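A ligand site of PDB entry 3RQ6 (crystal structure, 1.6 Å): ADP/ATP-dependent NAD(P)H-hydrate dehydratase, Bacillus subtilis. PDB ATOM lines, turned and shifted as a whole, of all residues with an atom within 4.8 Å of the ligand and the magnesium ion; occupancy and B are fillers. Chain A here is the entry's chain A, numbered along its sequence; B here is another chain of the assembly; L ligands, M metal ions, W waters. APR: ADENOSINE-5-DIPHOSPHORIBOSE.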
ATOM      1  N   MET A  42       6.239 -14.521  -2.949  1.00  0.00           N
ATOM      2  CA  MET A  42       7.218 -14.590  -4.019  1.00  0.00           C
ATOM      3  C   MET A  42       8.496 -13.864  -3.547  1.00  0.00           C
ATOM      4  O   MET A  42       8.934 -12.876  -4.175  1.00  0.00           O
ATOM      5  CB  MET A  42       6.657 -13.954  -5.278  1.00  0.00           C
ATOM      6  CG  MET A  42       5.474 -14.749  -5.781  1.00  0.00           C
ATOM      7  SD  MET A  42       4.793 -13.982  -7.287  1.00  0.00           S
ATOM      8  CE  MET A  42       4.159 -12.498  -6.682  1.00  0.00           C
ATOM      9  N   ALA A  45      12.338 -13.991  -5.928  1.00  0.00           N
ATOM     10  CA  ALA A  45      12.654 -13.093  -7.035  1.00  0.00           C
ATOM     11  C   ALA A  45      13.651 -11.996  -6.613  1.00  0.00           C
ATOM     12  O   ALA A  45      14.461 -11.573  -7.415  1.00  0.00           O
ATOM     13  CB  ALA A  45      11.376 -12.464  -7.598  1.00  0.00           C
ATOM     14  N   ASP A 131       9.339  -5.174 -14.750  1.00  0.00           N
ATOM     15  CA  ASP A 131       9.248  -6.598 -14.984  1.00  0.00           C
ATOM     16  C   ASP A 131       8.099  -7.167 -14.193  1.00  0.00           C
ATOM     17  O   ASP A 131       7.641  -6.560 -13.280  1.00  0.00           O
ATOM     18  CB  ASP A 131      10.584  -7.272 -14.606  1.00  0.00           C
ATOM     19  CG  ASP A 131      10.639  -8.739 -14.941  1.00  0.00           C
ATOM     20  OD1 ASP A 131       9.978  -9.125 -15.866  1.00  0.00           O
ATOM     21  OD2 ASP A 131      11.304  -9.467 -14.226  1.00  0.00           O
ATOM     22  N   HIS A 152       7.611 -11.670 -20.732  1.00  0.00           N
ATOM     23  CA  HIS A 152       7.418 -12.901 -21.473  1.00  0.00           C
ATOM     24  C   HIS A 152       6.105 -12.774 -22.255  1.00  0.00           C
ATOM     25  O   HIS A 152       5.330 -11.828 -22.067  1.00  0.00           O
ATOM     26  CB  HIS A 152       7.469 -14.177 -20.620  1.00  0.00           C
ATOM     27  CG  HIS A 152       6.268 -14.367 -19.735  1.00  0.00           C
ATOM     28  ND1 HIS A 152       6.364 -14.539 -18.367  1.00  0.00           N
ATOM     29  CD2 HIS A 152       4.950 -14.369 -20.007  1.00  0.00           C
ATOM     30  CE1 HIS A 152       5.153 -14.660 -17.844  1.00  0.00           C
ATOM     31  NE2 HIS A 152       4.274 -14.552 -18.817  1.00  0.00           N
ATOM     32  N   GLU A 155       2.881 -11.849 -20.479  1.00  0.00           N
ATOM     33  CA  GLU A 155       2.843 -10.488 -19.949  1.00  0.00           C
ATOM     34  C   GLU A 155       2.632  -9.504 -21.108  1.00  0.00           C
ATOM     35  O   GLU A 155       2.046  -8.459 -20.956  1.00  0.00           O
ATOM     36  CB  GLU A 155       4.113 -10.184 -19.157  1.00  0.00           C
ATOM     37  CG  GLU A 155       4.256 -11.082 -17.898  1.00  0.00           C
ATOM     38  CD  GLU A 155       5.621 -11.197 -17.292  1.00  0.00           C
ATOM     39  OE1 GLU A 155       6.626 -11.055 -18.015  1.00  0.00           O
ATOM     40  OE2 GLU A 155       5.652 -11.514 -16.076  1.00  0.00           O
ATOM     41  N   LYS A 189      10.781 -11.782 -24.299  1.00  0.00           N
ATOM     42  CA  LYS A 189      11.491 -12.985 -23.941  1.00  0.00           C
ATOM     43  C   LYS A 189      11.062 -14.191 -24.755  1.00  0.00           C
ATOM     44  O   LYS A 189       9.983 -14.202 -25.417  1.00  0.00           O
ATOM     45  CB  LYS A 189      11.262 -13.215 -22.453  1.00  0.00           C
ATOM     46  CG  LYS A 189      11.949 -12.236 -21.586  1.00  0.00           C
ATOM     47  CD  LYS A 189      11.316 -12.307 -20.150  1.00  0.00           C
ATOM     48  CE  LYS A 189      12.197 -11.733 -19.165  1.00  0.00           C
ATOM     49  NZ  LYS A 189      11.419 -11.367 -17.859  1.00  0.00           N
ATOM     50  N   GLY A 190      11.951 -15.178 -24.772  1.00  0.00           N
ATOM     51  CA  GLY A 190      11.772 -16.415 -25.495  1.00  0.00           C
ATOM     52  C   GLY A 190      13.041 -16.805 -26.207  1.00  0.00           C
ATOM     53  O   GLY A 190      14.022 -16.077 -26.207  1.00  0.00           O
ATOM     54  N   ASN A 191      13.025 -17.954 -26.842  1.00  0.00           N
ATOM     55  CA  ASN A 191      14.064 -18.282 -27.805  1.00  0.00           C
ATOM     56  C   ASN A 191      14.134 -17.079 -28.771  1.00  0.00           C
ATOM     57  O   ASN A 191      13.074 -16.567 -29.162  1.00  0.00           O
ATOM     58  CB  ASN A 191      13.650 -19.539 -28.558  1.00  0.00           C
ATOM     59  CG  ASN A 191      14.649 -19.945 -29.619  1.00  0.00           C
ATOM     60  OD1 ASN A 191      15.833 -19.899 -29.412  1.00  0.00           O
ATOM     61  ND2 ASN A 191      14.154 -20.307 -30.791  1.00  0.00           N
ATOM     62  N   THR A 193      15.140 -13.930 -28.135  1.00  0.00           N
ATOM     63  CA  THR A 193      14.585 -12.759 -27.434  1.00  0.00           C
ATOM     64  C   THR A 193      14.743 -11.537 -28.359  1.00  0.00           C
ATOM     65  O   THR A 193      15.788 -11.363 -29.006  1.00  0.00           O
ATOM     66  CB  THR A 193      15.296 -12.520 -26.106  1.00  0.00           C
ATOM     67  OG1 THR A 193      14.816 -13.506 -25.184  1.00  0.00           O
ATOM     68  CG2 THR A 193      15.014 -11.127 -25.547  1.00  0.00           C
ATOM     69  N   THR A 207      21.826 -16.035 -28.166  1.00  0.00           N
ATOM     70  CA  THR A 207      22.340 -16.969 -27.162  1.00  0.00           C
ATOM     71  C   THR A 207      21.182 -17.531 -26.336  1.00  0.00           C
ATOM     72  O   THR A 207      20.088 -16.951 -26.235  1.00  0.00           O
ATOM     73  CB  THR A 207      23.369 -16.287 -26.216  1.00  0.00           C
ATOM     74  OG1 THR A 207      22.685 -15.277 -25.488  1.00  0.00           O
ATOM     75  CG2 THR A 207      24.595 -15.737 -26.989  1.00  0.00           C
ATOM     76  N   GLY A 208      21.487 -18.604 -25.604  1.00  0.00           N
ATOM     77  CA  GLY A 208      20.536 -19.230 -24.748  1.00  0.00           C
ATOM     78  C   GLY A 208      20.002 -20.551 -25.291  1.00  0.00           C
ATOM     79  O   GLY A 208      20.231 -20.914 -26.462  1.00  0.00           O
ATOM     80  N   ASN A 209      19.285 -21.256 -24.429  1.00  0.00           N
ATOM     81  CA  ASN A 209      18.672 -22.521 -24.769  1.00  0.00           C
ATOM     82  C   ASN A 209      17.620 -22.881 -23.777  1.00  0.00           C
ATOM     83  O   ASN A 209      17.249 -22.057 -22.907  1.00  0.00           O
ATOM     84  CB  ASN A 209      19.735 -23.600 -24.859  1.00  0.00           C
ATOM     85  CG  ASN A 209      20.488 -23.776 -23.581  1.00  0.00           C
ATOM     86  OD1 ASN A 209      19.903 -23.722 -22.490  1.00  0.00           O
ATOM     87  ND2 ASN A 209      21.815 -24.003 -23.687  1.00  0.00           N
ATOM     88  N   GLY A 210      17.042 -24.084 -23.933  1.00  0.00           N
ATOM     89  CA  GLY A 210      15.907 -24.430 -23.109  1.00  0.00           C
ATOM     90  C   GLY A 210      16.210 -24.656 -21.634  1.00  0.00           C
ATOM     91  O   GLY A 210      15.290 -24.756 -20.822  1.00  0.00           O
ATOM     92  N   LEU A 212      17.010 -22.347 -19.897  1.00  0.00           N
ATOM     93  CA  LEU A 212      16.370 -21.129 -19.337  1.00  0.00           C
ATOM     94  C   LEU A 212      14.881 -21.186 -19.138  1.00  0.00           C
ATOM     95  O   LEU A 212      14.320 -20.304 -18.487  1.00  0.00           O
ATOM     96  CB  LEU A 212      16.707 -19.922 -20.194  1.00  0.00           C
ATOM     97  CG  LEU A 212      18.190 -19.552 -20.305  1.00  0.00           C
ATOM     98  CD1 LEU A 212      18.373 -18.508 -21.423  1.00  0.00           C
ATOM     99  CD2 LEU A 212      18.757 -19.039 -18.977  1.00  0.00           C
ATOM    100  N   ALA A 213      14.228 -22.230 -19.636  1.00  0.00           N
ATOM    101  CA  ALA A 213      12.791 -22.347 -19.604  1.00  0.00           C
ATOM    102  C   ALA A 213      12.358 -22.939 -18.254  1.00  0.00           C
ATOM    103  O   ALA A 213      11.816 -24.071 -18.182  1.00  0.00           O
ATOM    104  CB  ALA A 213      12.328 -23.214 -20.785  1.00  0.00           C
ATOM    105  N   LYS A 214      12.591 -22.160 -17.186  1.00  0.00           N
ATOM    106  CA  LYS A 214      12.276 -22.568 -15.826  1.00  0.00           C
ATOM    107  C   LYS A 214      12.181 -21.343 -14.970  1.00  0.00           C
ATOM    108  O   LYS A 214      12.856 -20.354 -15.246  1.00  0.00           O
ATOM    109  CB  LYS A 214      13.370 -23.502 -15.311  1.00  0.00           C
ATOM    110  CG  LYS A 214      13.020 -24.234 -14.030  1.00  0.00           C
ATOM    111  CD  LYS A 214      14.144 -25.164 -13.485  1.00  0.00           C
ATOM    112  CE  LYS A 214      14.505 -26.329 -14.444  1.00  0.00           C
ATOM    113  NZ  LYS A 214      15.748 -27.016 -13.937  1.00  0.00           N
ATOM    114  N   GLY A 215      11.374 -21.433 -13.904  1.00  0.00           N
ATOM    115  CA  GLY A 215      11.180 -20.322 -12.998  1.00  0.00           C
ATOM    116  C   GLY A 215      12.466 -19.691 -12.510  1.00  0.00           C
ATOM    117  O   GLY A 215      13.375 -20.351 -12.044  1.00  0.00           O
ATOM    118  N   GLY A 216      12.520 -18.377 -12.646  1.00  0.00           N
ATOM    119  CA  GLY A 216      13.536 -17.545 -11.982  1.00  0.00           C
ATOM    120  C   GLY A 216      14.565 -16.958 -12.905  1.00  0.00           C
ATOM    121  O   GLY A 216      15.315 -16.045 -12.529  1.00  0.00           O
ATOM    122  N   THR A 217      14.657 -17.498 -14.099  1.00  0.00           N
ATOM    123  CA  THR A 217      15.682 -17.050 -15.010  1.00  0.00           C
ATOM    124  C   THR A 217      15.450 -15.615 -15.528  1.00  0.00           C
ATOM    125  O   THR A 217      16.401 -14.880 -15.794  1.00  0.00           O
ATOM    126  CB  THR A 217      15.858 -18.002 -16.175  1.00  0.00           C
ATOM    127  OG1 THR A 217      14.630 -18.042 -16.927  1.00  0.00           O
ATOM    128  CG2 THR A 217      16.262 -19.443 -15.701  1.00  0.00           C
ATOM    129  N   GLY A 218      14.187 -15.197 -15.558  1.00  0.00           N
ATOM    130  CA  GLY A 218      13.855 -13.844 -15.932  1.00  0.00           C
ATOM    131  C   GLY A 218      14.116 -12.867 -14.800  1.00  0.00           C
ATOM    132  O   GLY A 218      14.539 -11.730 -15.045  1.00  0.00           O
ATOM    133  N   ASP A 219      13.847 -13.270 -13.553  1.00  0.00           N
ATOM    134  CA  ASP A 219      14.231 -12.438 -12.391  1.00  0.00           C
ATOM    135  C   ASP A 219      15.732 -12.186 -12.414  1.00  0.00           C
ATOM    136  O   ASP A 219      16.217 -11.045 -12.181  1.00  0.00           O
ATOM    137  CB  ASP A 219      13.854 -13.113 -11.092  1.00  0.00           C
ATOM    138  CG  ASP A 219      12.359 -13.398 -10.962  1.00  0.00           C
ATOM    139  OD1 ASP A 219      11.521 -12.677 -11.562  1.00  0.00           O
ATOM    140  OD2 ASP A 219      12.053 -14.360 -10.197  1.00  0.00           O
ATOM    141  N   LEU A 221      17.669 -12.194 -15.078  1.00  0.00           N
ATOM    142  CA  LEU A 221      17.923 -11.259 -16.180  1.00  0.00           C
ATOM    143  C   LEU A 221      17.611  -9.819 -15.814  1.00  0.00           C
ATOM    144  O   LEU A 221      18.355  -8.917 -16.123  1.00  0.00           O
ATOM    145  CB  LEU A 221      17.135 -11.658 -17.422  1.00  0.00           C
ATOM    146  CG  LEU A 221      17.213 -10.649 -18.574  1.00  0.00           C
ATOM    147  CD1 LEU A 221      18.690 -10.555 -19.119  1.00  0.00           C
ATOM    148  CD2 LEU A 221      16.270 -11.080 -19.715  1.00  0.00           C
ATOM    149  N   HIS A 246      23.434 -13.398 -20.410  1.00  0.00           N
ATOM    150  CA  HIS A 246      22.497 -14.266 -19.739  1.00  0.00           C
ATOM    151  C   HIS A 246      22.299 -15.561 -20.514  1.00  0.00           C
ATOM    152  O   HIS A 246      22.368 -16.649 -19.929  1.00  0.00           O
ATOM    153  CB  HIS A 246      21.189 -13.475 -19.534  1.00  0.00           C
ATOM    154  CG  HIS A 246      20.029 -14.233 -18.971  1.00  0.00           C
ATOM    155  ND1 HIS A 246      19.034 -14.753 -19.777  1.00  0.00           N
ATOM    156  CD2 HIS A 246      19.639 -14.456 -17.674  1.00  0.00           C
ATOM    157  CE1 HIS A 246      18.100 -15.284 -18.989  1.00  0.00           C
ATOM    158  NE2 HIS A 246      18.450 -15.125 -17.719  1.00  0.00           N
ATOM    159  N   ASP B  22      13.914 -28.726 -26.033  1.00  0.00           N
ATOM    160  CA  ASP B  22      14.058 -28.018 -27.292  1.00  0.00           C
ATOM    161  C   ASP B  22      14.319 -26.535 -27.159  1.00  0.00           C
ATOM    162  O   ASP B  22      13.793 -25.910 -26.253  1.00  0.00           O
ATOM    163  CB  ASP B  22      12.777 -28.140 -28.138  1.00  0.00           C
ATOM    164  CG  ASP B  22      12.741 -29.389 -28.966  1.00  0.00           C
ATOM    165  OD1 ASP B  22      11.921 -29.413 -29.909  1.00  0.00           O
ATOM    166  OD2 ASP B  22      13.494 -30.362 -28.690  1.00  0.00           O
ATOM    167  N   ALA B  23      15.049 -25.977 -28.130  1.00  0.00           N
ATOM    168  CA  ALA B  23      15.237 -24.519 -28.295  1.00  0.00           C
ATOM    169  C   ALA B  23      13.918 -23.762 -28.261  1.00  0.00           C
ATOM    170  O   ALA B  23      13.834 -22.664 -27.661  1.00  0.00           O
ATOM    171  CB  ALA B  23      15.955 -24.252 -29.614  1.00  0.00           C
ATOM    172  N   GLU B  24      12.883 -24.349 -28.845  1.00  0.00           N
ATOM    173  CA  GLU B  24      11.584 -23.670 -29.004  1.00  0.00           C
ATOM    174  C   GLU B  24      10.720 -23.746 -27.750  1.00  0.00           C
ATOM    175  O   GLU B  24       9.614 -23.221 -27.728  1.00  0.00           O
ATOM    176  CB  GLU B  24      10.751 -24.287 -30.154  1.00  0.00           C
ATOM    177  CG  GLU B  24      11.528 -24.839 -31.337  1.00  0.00           C
ATOM    178  CD  GLU B  24      12.445 -23.819 -31.973  1.00  0.00           C
ATOM    179  OE1 GLU B  24      12.205 -22.600 -31.721  1.00  0.00           O
ATOM    180  OE2 GLU B  24      13.398 -24.222 -32.697  1.00  0.00           O
ATOM    181  N   SER B  25      11.191 -24.402 -26.696  1.00  0.00           N
ATOM    182  CA  SER B  25      10.345 -24.641 -25.554  1.00  0.00           C
ATOM    183  C   SER B  25      10.322 -23.412 -24.619  1.00  0.00           C
ATOM    184  O   SER B  25      11.204 -22.555 -24.662  1.00  0.00           O
ATOM    185  CB  SER B  25      10.845 -25.850 -24.763  1.00  0.00           C
ATOM    186  OG  SER B  25      12.198 -25.688 -24.381  1.00  0.00           O
ATOM    187  N   HIS B  26       9.278 -23.355 -23.829  1.00  0.00           N
ATOM    188  CA  HIS B  26       9.092 -22.318 -22.822  1.00  0.00           C
ATOM    189  C   HIS B  26       8.720 -23.020 -21.534  1.00  0.00           C
ATOM    190  O   HIS B  26       8.428 -24.225 -21.540  1.00  0.00           O
ATOM    191  CB  HIS B  26       8.027 -21.288 -23.260  1.00  0.00           C
ATOM    192  CG  HIS B  26       6.724 -21.895 -23.667  1.00  0.00           C
ATOM    193  ND1 HIS B  26       5.585 -21.808 -22.889  1.00  0.00           N
ATOM    194  CD2 HIS B  26       6.365 -22.606 -24.773  1.00  0.00           C
ATOM    195  CE1 HIS B  26       4.583 -22.445 -23.487  1.00  0.00           C
ATOM    196  NE2 HIS B  26       5.043 -22.951 -24.621  1.00  0.00           N
ATOM    197  N   LYS B  27       8.725 -22.318 -20.406  1.00  0.00           N
ATOM    198  CA  LYS B  27       8.601 -23.087 -19.137  1.00  0.00           C
ATOM    199  C   LYS B  27       7.209 -23.802 -19.044  1.00  0.00           C
ATOM    200  O   LYS B  27       7.098 -24.889 -18.456  1.00  0.00           O
ATOM    201  CB  LYS B  27       8.928 -22.189 -17.949  1.00  0.00           C
ATOM    202  CG  LYS B  27       7.935 -21.197 -17.581  1.00  0.00           C
ATOM    203  CD  LYS B  27       8.561 -20.286 -16.482  1.00  0.00           C
ATOM    204  CE  LYS B  27       9.545 -19.282 -17.080  1.00  0.00           C
ATOM    205  NZ  LYS B  27       8.706 -18.385 -17.948  1.00  0.00           N
ATOM    206  N   LYS B  60       7.934 -24.773 -13.488  1.00  0.00           N
ATOM    207  CA  LYS B  60       7.763 -23.964 -12.249  1.00  0.00           C
ATOM    208  C   LYS B  60       7.501 -24.920 -11.078  1.00  0.00           C
ATOM    209  O   LYS B  60       6.931 -25.994 -11.300  1.00  0.00           O
ATOM    210  CB  LYS B  60       6.644 -22.920 -12.366  1.00  0.00           C
ATOM    211  CG  LYS B  60       7.034 -21.756 -13.267  1.00  0.00           C
ATOM    212  CD  LYS B  60       6.032 -20.640 -13.259  1.00  0.00           C
ATOM    213  CE  LYS B  60       4.895 -20.904 -14.231  1.00  0.00           C
ATOM    214  NZ  LYS B  60       3.889 -19.737 -14.207  1.00  0.00           N
ATOM    215  N   PRO B  78      15.749 -20.218  -4.407  1.00  0.00           N
ATOM    216  CA  PRO B  78      14.914 -19.006  -4.590  1.00  0.00           C
ATOM    217  C   PRO B  78      13.980 -19.055  -5.813  1.00  0.00           C
ATOM    218  O   PRO B  78      13.156 -18.172  -6.019  1.00  0.00           O
ATOM    219  CB  PRO B  78      15.961 -17.871  -4.720  1.00  0.00           C
ATOM    220  CG  PRO B  78      17.180 -18.595  -5.279  1.00  0.00           C
ATOM    221  CD  PRO B  78      17.180 -19.957  -4.581  1.00  0.00           C
ATOM    222  N   GLU B  79      14.120 -20.087  -6.631  1.00  0.00           N
ATOM    223  CA  GLU B  79      13.291 -20.257  -7.809  1.00  0.00           C
ATOM    224  C   GLU B  79      11.896 -20.798  -7.561  1.00  0.00           C
ATOM    225  O   GLU B  79      11.059 -20.653  -8.443  1.00  0.00           O
ATOM    226  CB  GLU B  79      13.993 -21.207  -8.796  1.00  0.00           C
ATOM    227  CG  GLU B  79      15.394 -20.764  -9.192  1.00  0.00           C
ATOM    228  CD  GLU B  79      16.553 -21.012  -8.189  1.00  0.00           C
ATOM    229  OE1 GLU B  79      16.369 -21.719  -7.156  1.00  0.00           O
ATOM    230  OE2 GLU B  79      17.667 -20.521  -8.535  1.00  0.00           O
ATOM    231  N   ALA B  80      11.639 -21.342  -6.364  1.00  0.00           N
ATOM    232  CA  ALA B  80      10.318 -21.828  -5.999  1.00  0.00           C
ATOM    233  C   ALA B  80       9.461 -20.692  -5.526  1.00  0.00           C
ATOM    234  O   ALA B  80       9.975 -19.674  -5.010  1.00  0.00           O
ATOM    235  CB  ALA B  80      10.437 -22.841  -4.847  1.00  0.00           C
ATOM    236  N   THR B  81       8.172 -20.809  -5.780  1.00  0.00           N
ATOM    237  CA  THR B  81       7.191 -19.949  -5.141  1.00  0.00           C
ATOM    238  C   THR B  81       6.325 -20.770  -4.221  1.00  0.00           C
ATOM    239  O   THR B  81       6.489 -21.958  -4.073  1.00  0.00           O
ATOM    240  CB  THR B  81       6.344 -19.142  -6.145  1.00  0.00           C
ATOM    241  OG1 THR B  81       5.587 -20.083  -6.921  1.00  0.00           O
ATOM    242  CG2 THR B  81       7.228 -18.216  -7.058  1.00  0.00           C
HETATM  243  N1  APR L   1      15.721 -20.423 -25.289  1.00  0.00           N
HETATM  244  C2  APR L   1      16.367 -19.314 -24.870  1.00  0.00           C
HETATM  245  N3  APR L   1      15.914 -18.558 -23.826  1.00  0.00           N
HETATM  246  C4  APR L   1      14.813 -18.951 -23.163  1.00  0.00           C
HETATM  247  C5  APR L   1      14.096 -20.141 -23.504  1.00  0.00           C
HETATM  248  C6  APR L   1      14.628 -20.896 -24.652  1.00  0.00           C
HETATM  249  N6  APR L   1      13.950 -21.991 -25.003  1.00  0.00           N
HETATM  250  N7  APR L   1      13.001 -20.285 -22.686  1.00  0.00           N
HETATM  251  C8  APR L   1      13.079 -19.239 -21.822  1.00  0.00           C
HETATM  252  N9  APR L   1      14.147 -18.472 -22.105  1.00  0.00           N
HETATM  253  C1' APR L   1      14.544 -17.259 -21.379  1.00  0.00           C
HETATM  254  C2' APR L   1      13.697 -16.047 -21.706  1.00  0.00           C
HETATM  255  O2' APR L   1      14.107 -15.412 -22.943  1.00  0.00           O
HETATM  256  C3' APR L   1      13.912 -15.221 -20.442  1.00  0.00           C
HETATM  257  O3' APR L   1      15.171 -14.569 -20.469  1.00  0.00           O
HETATM  258  O4' APR L   1      14.308 -17.478 -19.973  1.00  0.00           O
HETATM  259  C4' APR L   1      13.853 -16.265 -19.313  1.00  0.00           C
HETATM  260  C5' APR L   1      12.466 -16.484 -18.787  1.00  0.00           C
HETATM  261  O5' APR L   1      12.085 -15.335 -18.021  1.00  0.00           O
HETATM  262  PA  APR L   1      10.680 -15.253 -17.382  1.00  0.00           P
HETATM  263  O1A APR L   1      10.504 -13.839 -16.828  1.00  0.00           O
HETATM  264  O2A APR L   1       9.626 -15.889 -18.254  1.00  0.00           O
HETATM  265  O3A APR L   1      10.928 -16.264 -16.099  1.00  0.00           O
HETATM  266  PB  APR L   1      10.706 -15.827 -14.505  1.00  0.00           P
HETATM  267  O1B APR L   1       9.632 -14.719 -14.429  1.00  0.00           O
HETATM  268  O2B APR L   1      11.965 -15.654 -13.879  1.00  0.00           O
HETATM  269  O5D APR L   1      10.093 -17.178 -13.866  1.00  0.00           O
HETATM  270  C5D APR L   1       8.691 -17.448 -13.768  1.00  0.00           C
HETATM  271  O4D APR L   1       8.957 -18.469 -11.562  1.00  0.00           O
HETATM  272  O1D APR L   1      10.730 -18.478 -10.028  1.00  0.00           O
HETATM  273  C1D APR L   1       9.530 -17.845 -10.421  1.00  0.00           C
HETATM  274  O2D APR L   1       9.833 -15.515  -9.673  1.00  0.00           O
HETATM  275  C2D APR L   1       9.709 -16.372 -10.815  1.00  0.00           C
HETATM  276  O3D APR L   1       7.291 -15.859 -10.776  1.00  0.00           O
HETATM  277  C3D APR L   1       8.455 -16.130 -11.629  1.00  0.00           C
HETATM  278  C4D APR L   1       8.227 -17.471 -12.331  1.00  0.00           C
HETATM  279 MG    MG M   1       9.259 -13.133 -15.441  1.00  0.00          MG
HETATM  280  O   HOH W   1       9.025 -11.496 -16.601  1.00  0.00           O
HETATM  281  O   HOH W   2      16.978 -21.188 -27.557  1.00  0.00           O
HETATM  282  O   HOH W   3       5.451 -17.892 -10.379  1.00  0.00           O
HETATM  283  O   HOH W   4       6.829 -13.368 -12.142  1.00  0.00           O
HETATM  284  O   HOH W   5       7.675 -14.109 -16.527  1.00  0.00           O
HETATM  285  O   HOH W   6      16.030 -13.090 -22.549  1.00  0.00           O
HETATM  286  O   HOH W   7       9.910 -19.503 -20.528  1.00  0.00           O
HETATM  287  O   HOH W   8      10.833 -12.090 -14.325  1.00  0.00           O
HETATM  288  O   HOH W   9       7.721 -12.534 -14.329  1.00  0.00           O
HETATM  289  O   HOH W  10       9.699 -15.323  -6.547  1.00  0.00           O
HETATM  290  O   HOH W  11       7.905 -14.384  -8.405  1.00  0.00           O
HETATM  291  O   HOH W  12       9.008 -12.490 -10.773  1.00  0.00           O
HETATM  292  O   HOH W  13      11.230 -16.926  -7.571  1.00  0.00           O
HETATM  293  O   HOH W  14      10.985 -19.865 -25.425  1.00  0.00           O
HETATM  294  O   HOH W  15      16.666 -15.871 -23.766  1.00  0.00           O
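The backbone NH (N) of Asp 219 is in hydrogen-bond range of an oxygen (O2B) of the ligand (3.1 Å).
OD2 of Asp 219 sits at hydrogen-bond distance from O2D of the ligand (2.6 Å).
O2A of the ligand is in salt-bridge range of NZ of Lys 27 of chain B (2.7 Å).
The backbone carbonyl oxygen (O) of Glu 79 of chain B sits at hydrogen-bond distance from an oxygen (O1D) of the ligand (2.7 Å).
O of Ala 23 of chain B lies within hydrogen-bond range of N6 of the ligand, at 2.7 Å.
An oxygen (O2B) of the ligand sits at hydrogen-bond distance from the backbone NH (N) of Gly 218, 2.8 Å away.
A nitrogen (N6) of the ligand is in hydrogen-bond range of the backbone carbonyl oxygen (O) of Ser 25 of chain B (2.8 Å).
O1A of the ligand sits close to NZ of Lys 189, at 2.8 Å.
N of Gly 190 lies within hydrogen-bond range of O2' of the ligand, at 2.8 Å.
O of Gly 190 is in hydrogen-bond range of O2' of the ligand, 3.3 Å away.
The backbone NH (N) of Gly 216 sits at hydrogen-bond distance from an oxygen (O5D) of the ligand (3.0 Å).
O2' of the ligand lies within hydrogen-bond range of OG1 of Thr 193 (3.0 Å).
O2B of the ligand is in hydrogen-bond range of N of Thr 217 (3.3 Å).
OG1 of Thr 217 sits close to O4' of the ligand (3.1 Å).
Water W5 bridges O2A of the ligand (3.2 Å) and OE2 of Glu 155 (3.3 Å).
Water W1 lies within hydrogen-bond range of the side-chain carboxylate of Asp 131, the side-chain amino group of Lys 189 and the side-chain carboxylate of Glu 155.
Water W8 bridges the side-chain carboxylate of Asp 131 (2.7 Å) and the side-chain carboxylate of Asp 219 (2.9 Å).
Water W6 bridges an oxygen (O3') of the ligand (2.7 Å) and the side-chain hydroxyl of Thr 193 (2.9 Å).
Water W10 lies within hydrogen-bond range of the backbone NH (N) of Ala 45, an oxygen (O2D) of the ligand and the backbone carbonyl oxygen (O) of Met 42.
Water W12 lies within hydrogen-bond range of the side-chain carboxylate of Asp 219 and an oxygen (O2D) of the ligand.
Merely in contact with the magnesium ion: Lys 189 (3.7 Å).
The nearest printed residue that does not touch the magnesium ion is Glu 155 (4.004 Å).
The magnesium ion is bound by an oxygen (O1B) of the ligand (1.9 Å).
Water W9 binds the magnesium ion, 2.0 Å away.
O1A of the ligand is bound to the magnesium ion (2.0 Å).
The magnesium ion is bound by water W1, at 2.0 Å.
Water W5 binds the magnesium ion (2.2 Å).
Water W8 is bound to the magnesium ion, at 2.2 Å.
The magnesium ion has six donor atoms within binding distance.
A nitrogen (N1) of the ligand sits close to the backbone carbonyl oxygen of Asn 209, at 3.3 Å.
The backbone carbonyl oxygen (O) of Leu 212 sits close to an oxygen (O4') of the ligand.
Residues that only touch the ligand: Ala 45 (3.999 Å), His 152 (3.5 Å), Asn 191 (3.7 Å), Gly 208 (3.9 Å), Gly 210 (3.7 Å), Ala 213 (3.6 Å), Gly 215 (3.2 Å), Leu 221 (3.7 Å), His 246 (3.4 Å) and Lys 60 of chain B (3.97 Å).
Within 4 Å of the ligand: Ala 45, His 152, Lys 189, Gly 190, Asn 191, Thr 193, Gly 208, Asn 209, Gly 210, Leu 212, Ala 213, Gly 215, Gly 216, Thr 217, Gly 218, Asp 219, Leu 221, His 246, Ala 23 of chain B, Ser 25 of chain B, Lys 27 of chain B, Lys 60 of chain B and Glu 79 of chain B.
The nearest printed residue that does not touch the ligand is Thr 81 of chain B (4.1 Å).
OG of Ser 25 of chain B lies within hydrogen-bond range of O of Asp 22 of chain B, at 2.5 Å.
OD1 of Asp 131 is in salt-bridge range of NZ of Lys 189 (3.3 Å).
The backbone carbonyl oxygen of Gly 190 is in hydrogen-bond range of the side-chain hydroxyl of Thr 193 (2.9 Å).
O of Leu 212 is in hydrogen-bond range of OG1 of Thr 217, at 2.8 Å.
A ring nitrogen (NE2) of His 246 is in hydrogen-bond range of the backbone carbonyl oxygen (O) of Thr 217, 2.8 Å away.
The side-chain hydroxyl (OG1) of Thr 217 sits at hydrogen-bond distance from the backbone carbonyl oxygen (O) of Lys 214 (3.4 Å).
The side-chain carboxylate of Glu 155 sits at hydrogen-bond distance from the backbone NH of His 152 (3.0 Å).
The side-chain carboxylate (OE1) of Glu 24 of chain B lies within hydrogen-bond range of the side-chain amide nitrogen (ND2) of Asn 191 (3.1 Å).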
